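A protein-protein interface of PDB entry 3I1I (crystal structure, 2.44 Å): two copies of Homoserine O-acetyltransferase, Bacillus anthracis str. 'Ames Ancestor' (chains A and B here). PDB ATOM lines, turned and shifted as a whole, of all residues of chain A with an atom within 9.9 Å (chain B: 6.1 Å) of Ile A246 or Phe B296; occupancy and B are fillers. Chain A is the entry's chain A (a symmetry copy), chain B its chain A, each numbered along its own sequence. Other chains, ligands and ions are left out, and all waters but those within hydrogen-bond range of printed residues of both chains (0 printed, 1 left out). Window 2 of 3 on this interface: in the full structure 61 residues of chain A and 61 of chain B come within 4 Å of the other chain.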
ATOM      1  N   PRO A 242      14.362 -14.878  -7.227  1.00  0.00           N
ATOM      2  CA  PRO A 242      13.246 -15.227  -6.356  1.00  0.00           C
ATOM      3  C   PRO A 242      13.129 -16.733  -6.151  1.00  0.00           C
ATOM      4  O   PRO A 242      13.533 -17.540  -6.996  1.00  0.00           O
ATOM      5  CB  PRO A 242      12.019 -14.700  -7.122  1.00  0.00           C
ATOM      6  CG  PRO A 242      12.410 -14.772  -8.574  1.00  0.00           C
ATOM      7  CD  PRO A 242      13.928 -14.619  -8.614  1.00  0.00           C
ATOM      8  N   ARG A 243      12.547 -17.104  -5.029  1.00  0.00           N
ATOM      9  CA  ARG A 243      12.311 -18.504  -4.740  1.00  0.00           C
ATOM     10  C   ARG A 243      11.298 -19.122  -5.710  1.00  0.00           C
ATOM     11  O   ARG A 243      10.268 -18.573  -5.969  1.00  0.00           O
ATOM     12  CB  ARG A 243      11.827 -18.634  -3.299  1.00  0.00           C
ATOM     13  CG  ARG A 243      11.816 -20.057  -2.768  1.00  0.00           C
ATOM     14  CD  ARG A 243      11.458 -20.075  -1.256  1.00  0.00           C
ATOM     15  NE  ARG A 243      12.586 -19.694  -0.425  1.00  0.00           N
ATOM     16  CZ  ARG A 243      13.538 -20.530   0.004  1.00  0.00           C
ATOM     17  NH1 ARG A 243      13.506 -21.814  -0.305  1.00  0.00           N
ATOM     18  NH2 ARG A 243      14.533 -20.087   0.780  1.00  0.00           N
ATOM     19  N   ASN A 244      11.621 -20.288  -6.232  1.00  0.00           N
ATOM     20  CA  ASN A 244      10.684 -21.098  -7.007  1.00  0.00           C
ATOM     21  C   ASN A 244      10.008 -22.083  -6.041  1.00  0.00           C
ATOM     22  O   ASN A 244      10.652 -23.013  -5.561  1.00  0.00           O
ATOM     23  CB  ASN A 244      11.424 -21.838  -8.106  1.00  0.00           C
ATOM     24  CG  ASN A 244      10.529 -22.779  -8.899  1.00  0.00           C
ATOM     25  OD1 ASN A 244       9.455 -23.215  -8.451  1.00  0.00           O
ATOM     26  ND2 ASN A 244      10.983 -23.120 -10.080  1.00  0.00           N
ATOM     27  N   SER A 245       8.714 -21.881  -5.790  1.00  0.00           N
ATOM     28  CA  SER A 245       7.975 -22.680  -4.831  1.00  0.00           C
ATOM     29  C   SER A 245       7.342 -23.943  -5.412  1.00  0.00           C
ATOM     30  O   SER A 245       6.591 -24.627  -4.720  1.00  0.00           O
ATOM     31  CB  SER A 245       6.888 -21.827  -4.183  1.00  0.00           C
ATOM     32  OG  SER A 245       7.475 -20.738  -3.516  1.00  0.00           O
ATOM     33  N   ILE A 246       7.686 -24.270  -6.650  1.00  0.00           N
ATOM     34  CA  ILE A 246       7.140 -25.413  -7.331  1.00  0.00           C
ATOM     35  C   ILE A 246       8.203 -26.483  -7.492  1.00  0.00           C
ATOM     36  O   ILE A 246       7.926 -27.595  -7.218  1.00  0.00           O
ATOM     37  CB  ILE A 246       6.554 -25.002  -8.713  1.00  0.00           C
ATOM     38  CG1 ILE A 246       5.439 -23.964  -8.521  1.00  0.00           C
ATOM     39  CG2 ILE A 246       6.028 -26.209  -9.478  1.00  0.00           C
ATOM     40  CD1 ILE A 246       4.288 -24.429  -7.628  1.00  0.00           C
ATOM     41  N   GLU A 247       9.417 -26.167  -7.915  1.00  0.00           N
ATOM     42  CA  GLU A 247      10.428 -27.213  -8.166  1.00  0.00           C
ATOM     43  C   GLU A 247      10.578 -28.167  -6.956  1.00  0.00           C
ATOM     44  O   GLU A 247      10.616 -27.721  -5.791  1.00  0.00           O
ATOM     45  CB  GLU A 247      11.775 -26.611  -8.576  1.00  0.00           C
ATOM     46  CG  GLU A 247      12.460 -25.786  -7.485  1.00  0.00           C
ATOM     47  CD  GLU A 247      13.808 -25.178  -7.882  1.00  0.00           C
ATOM     48  OE1 GLU A 247      14.362 -25.504  -8.987  1.00  0.00           O
ATOM     49  OE2 GLU A 247      14.326 -24.372  -7.057  1.00  0.00           O
ATOM     50  N   VAL A 248      10.608 -29.479  -7.241  1.00  0.00           N
ATOM     51  CA  VAL A 248      10.684 -30.513  -6.224  1.00  0.00           C
ATOM     52  C   VAL A 248      12.093 -31.089  -6.062  1.00  0.00           C
ATOM     53  O   VAL A 248      12.428 -31.629  -5.044  1.00  0.00           O
ATOM     54  CB  VAL A 248       9.682 -31.692  -6.524  1.00  0.00           C
ATOM     55  CG1 VAL A 248       8.215 -31.174  -6.630  1.00  0.00           C
ATOM     56  CG2 VAL A 248      10.129 -32.487  -7.757  1.00  0.00           C
ATOM     57  N   GLU A 249      12.954 -30.939  -7.047  1.00  0.00           N
ATOM     58  CA  GLU A 249      14.236 -31.671  -7.007  1.00  0.00           C
ATOM     59  C   GLU A 249      15.130 -31.231  -5.848  1.00  0.00           C
ATOM     60  O   GLU A 249      15.752 -32.072  -5.205  1.00  0.00           O
ATOM     61  CB  GLU A 249      15.000 -31.612  -8.333  1.00  0.00           C
ATOM     62  CG  GLU A 249      16.342 -32.356  -8.339  1.00  0.00           C
ATOM     63  CD  GLU A 249      16.248 -33.821  -7.905  1.00  0.00           C
ATOM     64  OE1 GLU A 249      17.240 -34.331  -7.323  1.00  0.00           O
ATOM     65  OE2 GLU A 249      15.197 -34.467  -8.147  1.00  0.00           O
ATOM     66  N   PRO A 250      15.177 -29.931  -5.511  1.00  0.00           N
ATOM     67  CA  PRO A 250      15.966 -29.568  -4.302  1.00  0.00           C
ATOM     68  C   PRO A 250      15.553 -30.290  -2.981  1.00  0.00           C
ATOM     69  O   PRO A 250      16.382 -30.437  -2.082  1.00  0.00           O
ATOM     70  CB  PRO A 250      15.712 -28.052  -4.155  1.00  0.00           C
ATOM     71  CG  PRO A 250      15.354 -27.604  -5.607  1.00  0.00           C
ATOM     72  CD  PRO A 250      14.514 -28.756  -6.108  1.00  0.00           C
ATOM     73  N   TYR A 251      14.296 -30.736  -2.917  1.00  0.00           N
ATOM     74  CA  TYR A 251      13.705 -31.401  -1.753  1.00  0.00           C
ATOM     75  C   TYR A 251      14.051 -32.883  -1.685  1.00  0.00           C
ATOM     76  O   TYR A 251      13.618 -33.583  -0.767  1.00  0.00           O
ATOM     77  CB  TYR A 251      12.169 -31.236  -1.765  1.00  0.00           C
ATOM     78  CG  TYR A 251      11.746 -29.849  -1.431  1.00  0.00           C
ATOM     79  CD1 TYR A 251      11.337 -29.511  -0.143  1.00  0.00           C
ATOM     80  CD2 TYR A 251      11.847 -28.835  -2.366  1.00  0.00           C
ATOM     81  CE1 TYR A 251      10.982 -28.208   0.182  1.00  0.00           C
ATOM     82  CE2 TYR A 251      11.520 -27.529  -2.048  1.00  0.00           C
ATOM     83  CZ  TYR A 251      11.076 -27.225  -0.786  1.00  0.00           C
ATOM     84  OH  TYR A 251      10.750 -25.927  -0.497  1.00  0.00           O
ATOM     85  N   GLU A 252      14.859 -33.352  -2.631  1.00  0.00           N
ATOM     86  CA  GLU A 252      15.065 -34.779  -2.784  1.00  0.00           C
ATOM     87  C   GLU A 252      16.468 -35.218  -2.436  1.00  0.00           C
ATOM     88  O   GLU A 252      16.656 -36.336  -2.017  1.00  0.00           O
ATOM     89  CB  GLU A 252      14.675 -35.192  -4.210  1.00  0.00           C
ATOM     90  CG  GLU A 252      13.148 -35.086  -4.418  1.00  0.00           C
ATOM     91  CD  GLU A 252      12.669 -35.457  -5.820  1.00  0.00           C
ATOM     92  OE1 GLU A 252      13.493 -35.821  -6.703  1.00  0.00           O
ATOM     93  OE2 GLU A 252      11.439 -35.382  -6.039  1.00  0.00           O
ATOM     94  N   THR A 258      18.666 -25.315  -5.470  1.00  0.00           N
ATOM     95  CA  THR A 258      17.505 -24.512  -5.848  1.00  0.00           C
ATOM     96  C   THR A 258      17.868 -23.652  -7.045  1.00  0.00           C
ATOM     97  O   THR A 258      19.050 -23.510  -7.421  1.00  0.00           O
ATOM     98  CB  THR A 258      17.041 -23.556  -4.689  1.00  0.00           C
ATOM     99  OG1 THR A 258      18.085 -22.606  -4.381  1.00  0.00           O
ATOM    100  CG2 THR A 258      16.619 -24.335  -3.468  1.00  0.00           C
ATOM    101  N   SER A 259      16.870 -23.054  -7.660  1.00  0.00           N
ATOM    102  CA  SER A 259      17.144 -22.253  -8.844  1.00  0.00           C
ATOM    103  C   SER A 259      17.859 -20.978  -8.452  1.00  0.00           C
ATOM    104  O   SER A 259      18.675 -20.493  -9.209  1.00  0.00           O
ATOM    105  CB  SER A 259      15.855 -21.928  -9.588  1.00  0.00           C
ATOM    106  OG  SER A 259      14.961 -21.211  -8.756  1.00  0.00           O
ATOM    107  N   VAL B 166      -0.450 -23.777   8.768  1.00  0.00           N
ATOM    108  CA  VAL B 166      -0.850 -24.019   7.380  1.00  0.00           C
ATOM    109  C   VAL B 166      -1.490 -25.418   7.226  1.00  0.00           C
ATOM    110  O   VAL B 166      -2.575 -25.542   6.697  1.00  0.00           O
ATOM    111  CB  VAL B 166       0.357 -23.857   6.411  1.00  0.00           C
ATOM    112  CG1 VAL B 166       0.028 -24.381   5.028  1.00  0.00           C
ATOM    113  CG2 VAL B 166       0.775 -22.393   6.363  1.00  0.00           C
ATOM    114  N   HIS B 167      -0.832 -26.456   7.727  1.00  0.00           N
ATOM    115  CA  HIS B 167      -1.245 -27.805   7.398  1.00  0.00           C
ATOM    116  C   HIS B 167      -2.161 -28.497   8.371  1.00  0.00           C
ATOM    117  O   HIS B 167      -2.720 -29.505   8.012  1.00  0.00           O
ATOM    118  CB  HIS B 167      -0.030 -28.651   7.098  1.00  0.00           C
ATOM    119  CG  HIS B 167       0.660 -28.242   5.844  1.00  0.00           C
ATOM    120  ND1 HIS B 167       0.364 -28.798   4.612  1.00  0.00           N
ATOM    121  CD2 HIS B 167       1.583 -27.275   5.609  1.00  0.00           C
ATOM    122  CE1 HIS B 167       1.114 -28.223   3.682  1.00  0.00           C
ATOM    123  NE2 HIS B 167       1.853 -27.287   4.255  1.00  0.00           N
ATOM    124  N   ASP B 291       9.748 -22.896   3.163  1.00  0.00           N
ATOM    125  CA  ASP B 291       8.830 -22.232   2.242  1.00  0.00           C
ATOM    126  C   ASP B 291       7.432 -22.775   2.450  1.00  0.00           C
ATOM    127  O   ASP B 291       7.105 -23.865   1.942  1.00  0.00           O
ATOM    128  CB  ASP B 291       9.234 -22.571   0.816  1.00  0.00           C
ATOM    129  CG  ASP B 291       8.414 -21.824  -0.223  1.00  0.00           C
ATOM    130  OD1 ASP B 291       7.581 -20.982   0.186  1.00  0.00           O
ATOM    131  OD2 ASP B 291       8.636 -22.064  -1.456  1.00  0.00           O
ATOM    132  N   ILE B 292       6.619 -22.061   3.229  1.00  0.00           N
ATOM    133  CA  ILE B 292       5.264 -22.509   3.478  1.00  0.00           C
ATOM    134  C   ILE B 292       4.454 -22.555   2.157  1.00  0.00           C
ATOM    135  O   ILE B 292       3.533 -23.370   2.025  1.00  0.00           O
ATOM    136  CB  ILE B 292       4.526 -21.699   4.605  1.00  0.00           C
ATOM    137  CG1 ILE B 292       4.221 -20.274   4.164  1.00  0.00           C
ATOM    138  CG2 ILE B 292       5.301 -21.756   5.931  1.00  0.00           C
ATOM    139  CD1 ILE B 292       3.240 -19.549   5.070  1.00  0.00           C
ATOM    140  N   ALA B 293       4.825 -21.743   1.156  1.00  0.00           N
ATOM    141  CA  ALA B 293       4.184 -21.829  -0.184  1.00  0.00           C
ATOM    142  C   ALA B 293       4.551 -23.082  -0.957  1.00  0.00           C
ATOM    143  O   ALA B 293       3.914 -23.394  -1.945  1.00  0.00           O
ATOM    144  CB  ALA B 293       4.501 -20.579  -1.045  1.00  0.00           C
ATOM    145  N   HIS B 294       5.587 -23.796  -0.553  1.00  0.00           N
ATOM    146  CA  HIS B 294       5.953 -25.022  -1.279  1.00  0.00           C
ATOM    147  C   HIS B 294       4.802 -26.020  -1.223  1.00  0.00           C
ATOM    148  O   HIS B 294       4.290 -26.346  -0.163  1.00  0.00           O
ATOM    149  CB  HIS B 294       7.184 -25.691  -0.693  1.00  0.00           C
ATOM    150  CG  HIS B 294       7.594 -26.899  -1.450  1.00  0.00           C
ATOM    151  ND1 HIS B 294       7.936 -26.846  -2.788  1.00  0.00           N
ATOM    152  CD2 HIS B 294       7.669 -28.202  -1.090  1.00  0.00           C
ATOM    153  CE1 HIS B 294       8.236 -28.064  -3.206  1.00  0.00           C
ATOM    154  NE2 HIS B 294       8.078 -28.906  -2.199  1.00  0.00           N
ATOM    155  N   GLY B 295       4.391 -26.531  -2.353  1.00  0.00           N
ATOM    156  CA  GLY B 295       3.163 -27.328  -2.361  1.00  0.00           C
ATOM    157  C   GLY B 295       2.058 -26.590  -3.105  1.00  0.00           C
ATOM    158  O   GLY B 295       1.375 -27.177  -3.912  1.00  0.00           O
ATOM    159  N   PHE B 296       1.976 -25.286  -2.911  1.00  0.00           N
ATOM    160  CA  PHE B 296       0.830 -24.525  -3.277  1.00  0.00           C
ATOM    161  C   PHE B 296       1.137 -23.743  -4.528  1.00  0.00           C
ATOM    162  O   PHE B 296       2.241 -23.825  -5.053  1.00  0.00           O
ATOM    163  CB  PHE B 296       0.489 -23.585  -2.119  1.00  0.00           C
ATOM    164  CG  PHE B 296       0.056 -24.305  -0.864  1.00  0.00           C
ATOM    165  CD1 PHE B 296      -1.261 -24.647  -0.667  1.00  0.00           C
ATOM    166  CD2 PHE B 296       0.976 -24.635   0.117  1.00  0.00           C
ATOM    167  CE1 PHE B 296      -1.652 -25.312   0.471  1.00  0.00           C
ATOM    168  CE2 PHE B 296       0.595 -25.289   1.254  1.00  0.00           C
ATOM    169  CZ  PHE B 296      -0.716 -25.626   1.431  1.00  0.00           C
ATOM    170  N   SER B 297       0.177 -22.955  -4.995  1.00  0.00           N
ATOM    171  CA  SER B 297       0.385 -22.144  -6.178  1.00  0.00           C
ATOM    172  C   SER B 297       0.962 -20.797  -5.830  1.00  0.00           C
ATOM    173  O   SER B 297       1.480 -20.134  -6.677  1.00  0.00           O
ATOM    174  CB  SER B 297      -0.927 -21.968  -6.949  1.00  0.00           C
ATOM    175  OG  SER B 297      -1.915 -21.398  -6.137  1.00  0.00           O
ATOM    176  N   SER B 298       0.864 -20.389  -4.576  1.00  0.00           N
ATOM    177  CA  SER B 298       1.475 -19.136  -4.123  1.00  0.00           C
ATOM    178  C   SER B 298       1.449 -19.051  -2.603  1.00  0.00           C
ATOM    179  O   SER B 298       0.743 -19.841  -1.927  1.00  0.00           O
ATOM    180  CB  SER B 298       0.670 -17.953  -4.643  1.00  0.00           C
ATOM    181  OG  SER B 298      -0.608 -17.881  -3.996  1.00  0.00           O
ATOM    182  N   LEU B 299       2.187 -18.075  -2.072  1.00  0.00           N
ATOM    183  CA  LEU B 299       2.156 -17.781  -0.645  1.00  0.00           C
ATOM    184  C   LEU B 299       0.733 -17.483  -0.206  1.00  0.00           C
ATOM    185  O   LEU B 299       0.298 -17.997   0.821  1.00  0.00           O
ATOM    186  CB  LEU B 299       3.072 -16.609  -0.318  1.00  0.00           C
ATOM    187  CG  LEU B 299       3.160 -16.198   1.152  1.00  0.00           C
ATOM    188  CD1 LEU B 299       3.589 -17.382   2.046  1.00  0.00           C
ATOM    189  CD2 LEU B 299       4.114 -15.005   1.311  1.00  0.00           C
ATOM    190  N   GLU B 301      -2.037 -18.576  -1.417  1.00  0.00           N
ATOM    191  CA  GLU B 301      -2.798 -19.800  -1.277  1.00  0.00           C
ATOM    192  C   GLU B 301      -2.423 -20.545  -0.007  1.00  0.00           C
ATOM    193  O   GLU B 301      -3.294 -21.004   0.691  1.00  0.00           O
ATOM    194  CB  GLU B 301      -2.676 -20.733  -2.487  1.00  0.00           C
ATOM    195  CG  GLU B 301      -3.771 -21.829  -2.440  1.00  0.00           C
ATOM    196  CD  GLU B 301      -3.445 -23.117  -3.179  1.00  0.00           C
ATOM    197  OE1 GLU B 301      -2.557 -23.105  -4.075  1.00  0.00           O
ATOM    198  OE2 GLU B 301      -4.126 -24.132  -2.851  1.00  0.00           O
ATOM    199  N   ALA B 302      -1.139 -20.661   0.301  1.00  0.00           N
ATOM    200  CA  ALA B 302      -0.713 -21.374   1.499  1.00  0.00           C
ATOM    201  C   ALA B 302      -1.413 -20.745   2.712  1.00  0.00           C
ATOM    202  O   ALA B 302      -1.973 -21.441   3.546  1.00  0.00           O
ATOM    203  CB  ALA B 302       0.828 -21.347   1.652  1.00  0.00           C
ATOM    204  N   ASN B 305      -5.268 -21.194   4.014  1.00  0.00           N
ATOM    205  CA  ASN B 305      -5.647 -22.335   4.846  1.00  0.00           C
ATOM    206  C   ASN B 305      -5.558 -22.043   6.362  1.00  0.00           C
ATOM    207  O   ASN B 305      -6.195 -22.719   7.160  1.00  0.00           O
ATOM    208  CB  ASN B 305      -4.743 -23.523   4.520  1.00  0.00           C
ATOM    209  CG  ASN B 305      -4.928 -24.044   3.104  1.00  0.00           C
ATOM    210  OD1 ASN B 305      -5.868 -24.778   2.847  1.00  0.00           O
ATOM    211  ND2 ASN B 305      -4.008 -23.702   2.189  1.00  0.00           N
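Among the printed residues, merely in contact across the chains: Ile A246 with Phe B296 (3.3 Å), Tyr A251 with His B294 (3.4 Å), Arg A243 with Asp B291 (3.5 Å), Glu A247 with His B294 (3.5 Å), Ser A245 with Gly B295 (3.8 Å), Ser A245 with Ala B293 (3.9 Å) and Tyr A251 with Asp B291 (3.9 Å).
No position is printed for both chains.
OD1 of Asp B291 sits at hydrogen-bond distance from N of Ala B293 (3.0 Å).
OD1 of Asn A244 sits at hydrogen-bond distance from N of Ile A246 (2.7 Å).
The backbone NH (N) of Glu A247 is in hydrogen-bond range of the side-chain amide oxygen (OD1) of Asn A244, 3.0 Å away.
OE2 of Glu A247 is in hydrogen-bond range of N of Ser A259, 2.9 Å away.
Of the 14 printed residues of chain B, 5 touch a printed residue of chain A.
Hydrophobic or aromatic side chains of chain B that line the printed part of chain A: Ala B293 and His B294.
Along chain B the printed residues that touch a printed residue of chain A span positions 291 to 296.
Phe B296 touches one residue of chain A.
No residue of chain A comes within 4 Å of Ser B297.
Of the printed residues of chain A, Asp B291 touches Arg A243, Ser A245 and Tyr A251.
Of the printed residues of chain B, Arg A243 touches Asp B291.
Printed residues of chain A within 4 Å of His B294: Ser A245 (3.2 Å), Glu A247 (3.5 Å) and Tyr A251 (3.4 Å).
Ser B298 touches none of the printed residues of chain A.
Ile B292 touches none of the printed residues of chain A.
The nearest residue of chain B that does not touch Ile A246 is His B294 (4.1 Å).
The side-chain carboxylate (OD2) of Asp B291 is in hydrogen-bond range of the side-chain hydroxyl (OG) of Ser A245 (2.7 Å).
O of Ser A245 sits at hydrogen-bond distance from ND1 of His B294 (3.2 Å).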
